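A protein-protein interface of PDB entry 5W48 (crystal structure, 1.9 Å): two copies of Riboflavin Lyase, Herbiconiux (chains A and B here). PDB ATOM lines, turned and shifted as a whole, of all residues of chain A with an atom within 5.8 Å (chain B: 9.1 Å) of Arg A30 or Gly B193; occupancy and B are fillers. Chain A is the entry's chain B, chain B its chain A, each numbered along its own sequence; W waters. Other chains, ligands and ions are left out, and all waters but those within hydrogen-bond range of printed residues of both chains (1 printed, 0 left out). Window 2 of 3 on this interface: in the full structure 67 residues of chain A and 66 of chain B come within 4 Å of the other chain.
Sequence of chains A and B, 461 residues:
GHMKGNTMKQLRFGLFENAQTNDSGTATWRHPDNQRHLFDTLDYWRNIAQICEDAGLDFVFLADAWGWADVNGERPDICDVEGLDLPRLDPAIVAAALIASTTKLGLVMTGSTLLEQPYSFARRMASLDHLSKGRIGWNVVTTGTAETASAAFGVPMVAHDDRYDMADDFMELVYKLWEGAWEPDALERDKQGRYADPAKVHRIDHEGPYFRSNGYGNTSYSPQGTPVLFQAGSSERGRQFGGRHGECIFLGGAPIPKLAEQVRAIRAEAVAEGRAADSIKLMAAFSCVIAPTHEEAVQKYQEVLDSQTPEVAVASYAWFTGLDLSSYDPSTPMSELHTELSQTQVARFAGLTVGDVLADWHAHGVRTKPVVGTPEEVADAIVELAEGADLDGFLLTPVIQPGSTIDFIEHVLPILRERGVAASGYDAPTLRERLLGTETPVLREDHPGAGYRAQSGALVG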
ATOM      1  N   ALA A  27     -27.279 -17.760  11.189  1.00  0.00           N
ATOM      2  CA  ALA A  27     -26.561 -16.578  11.651  1.00  0.00           C
ATOM      3  C   ALA A  27     -25.829 -16.830  12.960  1.00  0.00           C
ATOM      4  O   ALA A  27     -26.285 -16.393  14.023  1.00  0.00           O
ATOM      5  CB  ALA A  27     -27.520 -15.399  11.814  1.00  0.00           C
ATOM      6  N   THR A  28     -24.676 -17.497  12.889  1.00  0.00           N
ATOM      7  CA  THR A  28     -23.870 -17.794  14.063  1.00  0.00           C
ATOM      8  C   THR A  28     -22.700 -16.823  14.231  1.00  0.00           C
ATOM      9  O   THR A  28     -21.717 -17.159  14.899  1.00  0.00           O
ATOM     10  CB  THR A  28     -23.358 -19.227  13.977  1.00  0.00           C
ATOM     11  OG1 THR A  28     -22.696 -19.395  12.724  1.00  0.00           O
ATOM     12  CG2 THR A  28     -24.519 -20.216  14.057  1.00  0.00           C
ATOM     13  N   TRP A  29     -22.801 -15.619  13.659  1.00  0.00           N
ATOM     14  CA  TRP A  29     -21.706 -14.650  13.726  1.00  0.00           C
ATOM     15  C   TRP A  29     -21.347 -14.275  15.163  1.00  0.00           C
ATOM     16  O   TRP A  29     -20.224 -13.823  15.423  1.00  0.00           O
ATOM     17  CB  TRP A  29     -22.083 -13.385  12.948  1.00  0.00           C
ATOM     18  CG  TRP A  29     -23.187 -12.556  13.618  1.00  0.00           C
ATOM     19  CD1 TRP A  29     -24.525 -12.817  13.610  1.00  0.00           C
ATOM     20  CD2 TRP A  29     -23.018 -11.346  14.373  1.00  0.00           C
ATOM     21  NE1 TRP A  29     -25.203 -11.845  14.308  1.00  0.00           N
ATOM     22  CE2 TRP A  29     -24.300 -10.932  14.792  1.00  0.00           C
ATOM     23  CE3 TRP A  29     -21.908 -10.572  14.732  1.00  0.00           C
ATOM     24  CZ2 TRP A  29     -24.505  -9.777  15.559  1.00  0.00           C
ATOM     25  CZ3 TRP A  29     -22.109  -9.427  15.495  1.00  0.00           C
ATOM     26  CH2 TRP A  29     -23.400  -9.041  15.903  1.00  0.00           C
ATOM     27  N   ARG A  30     -22.297 -14.400  16.098  1.00  0.00           N
ATOM     28  CA  ARG A  30     -22.064 -14.039  17.493  1.00  0.00           C
ATOM     29  C   ARG A  30     -21.225 -15.053  18.256  1.00  0.00           C
ATOM     30  O   ARG A  30     -20.801 -14.752  19.377  1.00  0.00           O
ATOM     31  CB  ARG A  30     -23.391 -13.853  18.243  1.00  0.00           C
ATOM     32  CG  ARG A  30     -24.235 -12.679  17.774  1.00  0.00           C
ATOM     33  CD  ARG A  30     -25.575 -12.653  18.517  1.00  0.00           C
ATOM     34  NE  ARG A  30     -26.494 -11.638  17.993  1.00  0.00           N
ATOM     35  CZ  ARG A  30     -26.492 -10.363  18.374  1.00  0.00           C
ATOM     36  NH1 ARG A  30     -25.605  -9.945  19.268  1.00  0.00           N
ATOM     37  NH2 ARG A  30     -27.374  -9.508  17.874  1.00  0.00           N
ATOM     38  N   HIS A  31     -20.985 -16.227  17.689  1.00  0.00           N
ATOM     39  CA  HIS A  31     -20.130 -17.213  18.335  1.00  0.00           C
ATOM     40  C   HIS A  31     -18.733 -16.630  18.533  1.00  0.00           C
ATOM     41  O   HIS A  31     -18.180 -16.029  17.600  1.00  0.00           O
ATOM     42  CB  HIS A  31     -20.069 -18.483  17.489  1.00  0.00           C
ATOM     43  CG  HIS A  31     -19.319 -19.608  18.131  1.00  0.00           C
ATOM     44  ND1 HIS A  31     -17.945 -19.618  18.247  1.00  0.00           N
ATOM     45  CD2 HIS A  31     -19.750 -20.776  18.664  1.00  0.00           C
ATOM     46  CE1 HIS A  31     -17.562 -20.739  18.831  1.00  0.00           C
ATOM     47  NE2 HIS A  31     -18.638 -21.458  19.098  1.00  0.00           N
ATOM     48  N   PRO A  32     -18.132 -16.788  19.718  1.00  0.00           N
ATOM     49  CA  PRO A  32     -16.859 -16.092  20.011  1.00  0.00           C
ATOM     50  C   PRO A  32     -15.714 -16.429  19.064  1.00  0.00           C
ATOM     51  O   PRO A  32     -14.767 -15.636  18.948  1.00  0.00           O
ATOM     52  CB  PRO A  32     -16.526 -16.541  21.443  1.00  0.00           C
ATOM     53  CG  PRO A  32     -17.733 -17.272  21.967  1.00  0.00           C
ATOM     54  CD  PRO A  32     -18.785 -17.341  20.919  1.00  0.00           C
ATOM     55  N   ASN A  34     -16.131 -17.114  15.750  1.00  0.00           N
ATOM     56  CA  ASN A  34     -16.476 -16.822  14.368  1.00  0.00           C
ATOM     57  C   ASN A  34     -15.822 -15.515  13.954  1.00  0.00           C
ATOM     58  O   ASN A  34     -15.981 -14.491  14.625  1.00  0.00           O
ATOM     59  CB  ASN A  34     -17.988 -16.738  14.193  1.00  0.00           C
ATOM     60  CG  ASN A  34     -18.443 -17.337  12.887  1.00  0.00           C
ATOM     61  OD1 ASN A  34     -17.641 -17.537  11.973  1.00  0.00           O
ATOM     62  ND2 ASN A  34     -19.733 -17.643  12.792  1.00  0.00           N
ATOM     63  N   VAL A  81     -30.074  -6.203  12.468  1.00  0.00           N
ATOM     64  CA  VAL A  81     -29.620  -6.525  13.819  1.00  0.00           C
ATOM     65  C   VAL A  81     -28.764  -7.790  13.824  1.00  0.00           C
ATOM     66  O   VAL A  81     -27.814  -7.897  14.610  1.00  0.00           O
ATOM     67  CB  VAL A  81     -30.818  -6.643  14.780  1.00  0.00           C
ATOM     68  CG1 VAL A  81     -30.378  -7.240  16.113  1.00  0.00           C
ATOM     69  CG2 VAL A  81     -31.466  -5.282  14.998  1.00  0.00           C
ATOM     70  N   GLU A  82     -29.044  -8.739  12.928  1.00  0.00           N
ATOM     71  CA  GLU A  82     -28.299  -9.992  12.867  1.00  0.00           C
ATOM     72  C   GLU A  82     -27.487 -10.176  11.586  1.00  0.00           C
ATOM     73  O   GLU A  82     -26.869 -11.231  11.418  1.00  0.00           O
ATOM     74  CB  GLU A  82     -29.253 -11.177  13.039  1.00  0.00           C
ATOM     75  CG  GLU A  82     -30.053 -11.141  14.354  1.00  0.00           C
ATOM     76  CD  GLU A  82     -29.180 -11.370  15.574  1.00  0.00           C
ATOM     77  OE1 GLU A  82     -29.619 -11.043  16.702  1.00  0.00           O
ATOM     78  OE2 GLU A  82     -28.058 -11.900  15.406  1.00  0.00           O
ATOM     79  N   SER A 307     -25.477 -19.969  19.884  1.00  0.00           N
ATOM     80  CA  SER A 307     -25.006 -18.618  19.607  1.00  0.00           C
ATOM     81  C   SER A 307     -25.937 -17.846  18.678  1.00  0.00           C
ATOM     82  O   SER A 307     -25.777 -16.628  18.546  1.00  0.00           O
ATOM     83  CB  SER A 307     -23.605 -18.668  18.995  1.00  0.00           C
ATOM     84  OG  SER A 307     -23.671 -19.119  17.655  1.00  0.00           O
ATOM     85  N   THR A 309     -29.413 -16.145  17.571  1.00  0.00           N
ATOM     86  CA  THR A 309     -30.575 -15.552  18.228  1.00  0.00           C
ATOM     87  C   THR A 309     -31.849 -16.326  17.891  1.00  0.00           C
ATOM     88  O   THR A 309     -32.084 -16.639  16.716  1.00  0.00           O
ATOM     89  CB  THR A 309     -30.712 -14.096  17.793  1.00  0.00           C
ATOM     90  OG1 THR A 309     -29.543 -13.370  18.197  1.00  0.00           O
ATOM     91  CG2 THR A 309     -31.969 -13.455  18.395  1.00  0.00           C
ATOM     92  N   GLU B 188     -21.980  -2.077  13.174  1.00  0.00           N
ATOM     93  CA  GLU B 188     -21.468  -2.092  14.542  1.00  0.00           C
ATOM     94  C   GLU B 188     -20.721  -3.371  14.886  1.00  0.00           C
ATOM     95  O   GLU B 188     -19.658  -3.310  15.517  1.00  0.00           O
ATOM     96  CB  GLU B 188     -22.619  -1.882  15.537  1.00  0.00           C
ATOM     97  CG  GLU B 188     -23.431  -0.620  15.223  1.00  0.00           C
ATOM     98  CD  GLU B 188     -24.641  -0.403  16.140  1.00  0.00           C
ATOM     99  OE1 GLU B 188     -25.052  -1.323  16.881  1.00  0.00           O
ATOM    100  OE2 GLU B 188     -25.193   0.712  16.109  1.00  0.00           O
ATOM    101  N   ARG B 189     -21.261  -4.526  14.479  1.00  0.00           N
ATOM    102  CA  ARG B 189     -20.594  -5.830  14.606  1.00  0.00           C
ATOM    103  C   ARG B 189     -20.165  -6.114  16.049  1.00  0.00           C
ATOM    104  O   ARG B 189     -19.088  -6.648  16.321  1.00  0.00           O
ATOM    105  CB  ARG B 189     -19.420  -5.923  13.628  1.00  0.00           C
ATOM    106  CG  ARG B 189     -19.896  -5.902  12.184  1.00  0.00           C
ATOM    107  CD  ARG B 189     -18.765  -6.008  11.177  1.00  0.00           C
ATOM    108  NE  ARG B 189     -18.101  -4.727  10.982  1.00  0.00           N
ATOM    109  CZ  ARG B 189     -17.225  -4.489  10.016  1.00  0.00           C
ATOM    110  NH1 ARG B 189     -16.899  -5.455   9.162  1.00  0.00           N
ATOM    111  NH2 ARG B 189     -16.672  -3.294   9.908  1.00  0.00           N
ATOM    112  N   ASP B 190     -21.033  -5.780  16.984  1.00  0.00           N
ATOM    113  CA  ASP B 190     -20.823  -6.088  18.392  1.00  0.00           C
ATOM    114  C   ASP B 190     -21.542  -7.403  18.709  1.00  0.00           C
ATOM    115  O   ASP B 190     -22.775  -7.468  18.676  1.00  0.00           O
ATOM    116  CB  ASP B 190     -21.321  -4.927  19.257  1.00  0.00           C
ATOM    117  CG  ASP B 190     -21.237  -5.214  20.754  1.00  0.00           C
ATOM    118  OD1 ASP B 190     -20.529  -6.162  21.166  1.00  0.00           O
ATOM    119  OD2 ASP B 190     -21.877  -4.467  21.523  1.00  0.00           O
ATOM    120  N   LYS B 191     -20.766  -8.462  18.979  1.00  0.00           N
ATOM    121  CA  LYS B 191     -21.355  -9.790  19.192  1.00  0.00           C
ATOM    122  C   LYS B 191     -22.296  -9.826  20.391  1.00  0.00           C
ATOM    123  O   LYS B 191     -23.198 -10.673  20.439  1.00  0.00           O
ATOM    124  CB  LYS B 191     -20.246 -10.848  19.352  1.00  0.00           C
ATOM    125  CG  LYS B 191     -19.396 -11.063  18.079  1.00  0.00           C
ATOM    126  CD  LYS B 191     -18.434 -12.255  18.222  1.00  0.00           C
ATOM    127  CE  LYS B 191     -17.589 -12.467  16.964  1.00  0.00           C
ATOM    128  NZ  LYS B 191     -16.692 -13.666  17.130  1.00  0.00           N
ATOM    129  N   GLN B 192     -22.122  -8.925  21.356  1.00  0.00           N
ATOM    130  CA  GLN B 192     -23.075  -8.780  22.453  1.00  0.00           C
ATOM    131  C   GLN B 192     -24.083  -7.665  22.206  1.00  0.00           C
ATOM    132  O   GLN B 192     -24.902  -7.379  23.085  1.00  0.00           O
ATOM    133  CB  GLN B 192     -22.342  -8.526  23.779  1.00  0.00           C
ATOM    134  CG  GLN B 192     -21.702  -9.760  24.409  1.00  0.00           C
ATOM    135  CD  GLN B 192     -20.460 -10.221  23.669  1.00  0.00           C
ATOM    136  OE1 GLN B 192     -20.307 -11.405  23.369  1.00  0.00           O
ATOM    137  NE2 GLN B 192     -19.564  -9.285  23.370  1.00  0.00           N
ATOM    138  N   GLY B 193     -24.038  -7.019  21.043  1.00  0.00           N
ATOM    139  CA  GLY B 193     -24.962  -5.944  20.740  1.00  0.00           C
ATOM    140  C   GLY B 193     -25.685  -6.174  19.430  1.00  0.00           C
ATOM    141  O   GLY B 193     -26.391  -7.171  19.285  1.00  0.00           O
ATOM    142  N   ARG B 194     -25.511  -5.264  18.475  1.00  0.00           N
ATOM    143  CA  ARG B 194     -26.095  -5.360  17.143  1.00  0.00           C
ATOM    144  C   ARG B 194     -25.019  -5.582  16.083  1.00  0.00           C
ATOM    145  O   ARG B 194     -23.885  -5.113  16.212  1.00  0.00           O
ATOM    146  CB  ARG B 194     -26.861  -4.083  16.777  1.00  0.00           C
ATOM    147  CG  ARG B 194     -28.076  -3.797  17.638  1.00  0.00           C
ATOM    148  CD  ARG B 194     -28.845  -2.591  17.114  1.00  0.00           C
ATOM    149  NE  ARG B 194     -28.049  -1.364  17.113  1.00  0.00           N
ATOM    150  CZ  ARG B 194     -28.572  -0.142  17.170  1.00  0.00           C
ATOM    151  NH1 ARG B 194     -29.887   0.012  17.243  1.00  0.00           N
ATOM    152  NH2 ARG B 194     -27.784   0.927  17.170  1.00  0.00           N
ATOM    153  N   TYR B 195     -25.396  -6.285  15.012  1.00  0.00           N
ATOM    154  CA  TYR B 195     -24.551  -6.318  13.819  1.00  0.00           C
ATOM    155  C   TYR B 195     -24.548  -4.959  13.129  1.00  0.00           C
ATOM    156  O   TYR B 195     -23.487  -4.371  12.884  1.00  0.00           O
ATOM    157  CB  TYR B 195     -25.046  -7.396  12.852  1.00  0.00           C
ATOM    158  CG  TYR B 195     -24.152  -7.563  11.646  1.00  0.00           C
ATOM    159  CD1 TYR B 195     -24.427  -6.917  10.435  1.00  0.00           C
ATOM    160  CD2 TYR B 195     -23.026  -8.372  11.724  1.00  0.00           C
ATOM    161  CE1 TYR B 195     -23.578  -7.097   9.326  1.00  0.00           C
ATOM    162  CE2 TYR B 195     -22.187  -8.542  10.647  1.00  0.00           C
ATOM    163  CZ  TYR B 195     -22.458  -7.913   9.459  1.00  0.00           C
ATOM    164  OH  TYR B 195     -21.582  -8.126   8.422  1.00  0.00           O
ATOM    165  N   ALA B 196     -25.733  -4.450  12.803  1.00  0.00           N
ATOM    166  CA  ALA B 196     -25.879  -3.153  12.155  1.00  0.00           C
ATOM    167  C   ALA B 196     -27.070  -2.429  12.764  1.00  0.00           C
ATOM    168  O   ALA B 196     -27.997  -3.055  13.282  1.00  0.00           O
ATOM    169  CB  ALA B 196     -26.083  -3.287  10.647  1.00  0.00           C
ATOM    170  N   ASP B 197     -27.036  -1.103  12.703  1.00  0.00           N
ATOM    171  CA  ASP B 197     -28.172  -0.313  13.167  1.00  0.00           C
ATOM    172  C   ASP B 197     -29.191  -0.228  12.040  1.00  0.00           C
ATOM    173  O   ASP B 197     -28.921   0.421  11.022  1.00  0.00           O
ATOM    174  CB  ASP B 197     -27.700   1.074  13.603  1.00  0.00           C
ATOM    175  CG  ASP B 197     -28.844   1.989  14.035  1.00  0.00           C
ATOM    176  OD1 ASP B 197     -28.542   3.134  14.426  1.00  0.00           O
ATOM    177  OD2 ASP B 197     -30.028   1.587  13.981  1.00  0.00           O
HETATM  178  O   HOH W   1     -19.050 -13.699  21.668  1.00  0.00           O
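No position is printed for both chains.
Of the 15 pairs that touch across the chains among the printed residues, none has its exchanged pair printed and touching as well.
The side-chain carboxylate (OE2) of Glu B188 lies within salt-bridge range of the guanidinium group (NH2) of Arg B194 (2.8 Å).
The backbone NH (N) of Gln B192 lies close to the side-chain carboxylate (OD1) of Asp B190 (3.2 Å).
The guanidinium group (NH2) of Arg B194 lies within salt-bridge range of the side-chain carboxylate (OD1) of Asp B197 (3.6 Å).
ND2 of Asn A34 is in hydrogen-bond range of O of Thr A28 (2.9 Å).
The indole nitrogen of Trp A29 sits at hydrogen-bond distance from the side-chain carboxylate of Glu A82, at 3.1 Å.
OE1 of Glu A82 lies within hydrogen-bond range of OG1 of Thr A309, 2.8 Å away.
Among the printed residues, merely in contact across the chains: Trp A29 with Asp B190 (3.2 Å), Trp A29 with Lys B191 (3.3 Å), Trp A29 with Tyr B195 (3.5 Å), Arg A30 with Asp B190 (3.8 Å), Trp A29 with Arg B194 (3.8 Å), Val A81 with Ala B196 (3.9 Å), Trp A29 with Arg B189 (3.9 Å), Glu A82 with Tyr B195 (3.9 Å) and Val A81 with Arg B194 (3.9 Å).
Water W1 bridges the backbone carbonyl oxygen (O) of Arg A30 (3.1 Å) and the side-chain amide oxygen (OE1) of Gln B192 (3.1 Å).
O of Lys B191 lies within hydrogen-bond range of NH1 of Arg A30, at 2.8 Å.
The backbone carbonyl oxygen of His A31 lies within hydrogen-bond range of the side-chain amino group of Lys B191 (2.8 Å).
NZ of Lys B191 lies within hydrogen-bond range of O of Pro A32 (3.3 Å).
NZ of Lys B191 sits at hydrogen-bond distance from O of Asn A34, 2.7 Å away.
The guanidinium group of Arg A30 is in hydrogen-bond range of the backbone carbonyl oxygen of Gly B193, at 2.9 Å.
The backbone NH of Tyr B195 is in hydrogen-bond range of the backbone carbonyl oxygen of Val A81, 2.9 Å away.
Of the 11 printed residues of chain A, 7 touch a printed residue of chain B.
Hydrophobic or aromatic side chains of chain A within 4 Å of the printed part of chain B: Trp A29.
Of the 10 printed residues of chain B, 7 touch a printed residue of chain A.
Hydrophobic or aromatic side chains of chain B within 4 Å of the printed part of chain A: Tyr B195.
Among the printed residues, 15 pairs touch across the chains.
Among the printed residues, no Asp or Glu carboxylate lies within 4 Å of a Lys or Arg side-chain nitrogen of the other chain.
Thr A28 touches none of the printed residues of chain B.
Trp A29 touches five residues of chain B.
Of the printed residues of chain B, Arg A30 touches Asp B190 (3.8 Å), Lys B191 (2.8 Å) and Gly B193 (2.9 Å).
Printed residues of chain B within 4 Å of Pro A32: Lys B191 (3.3 Å).
Of the printed residues of chain A, Arg B189 touches Trp A29.
Of the printed residues of chain A, Lys B191 touches Trp A29, Arg A30, His A31, Pro A32 and Asn A34.
Gly B193 touches just one residue of chain A: Arg A30 (2.9 Å).
Printed residues of chain A within 4 Å of Tyr B195: Trp A29, Val A81 and Glu A82.
Printed residues of chain A within 4 Å of Ala B196: Val A81.
The nearest printed residue of chain B that does not touch Arg A30 is Gln B192 (4.02 Å).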
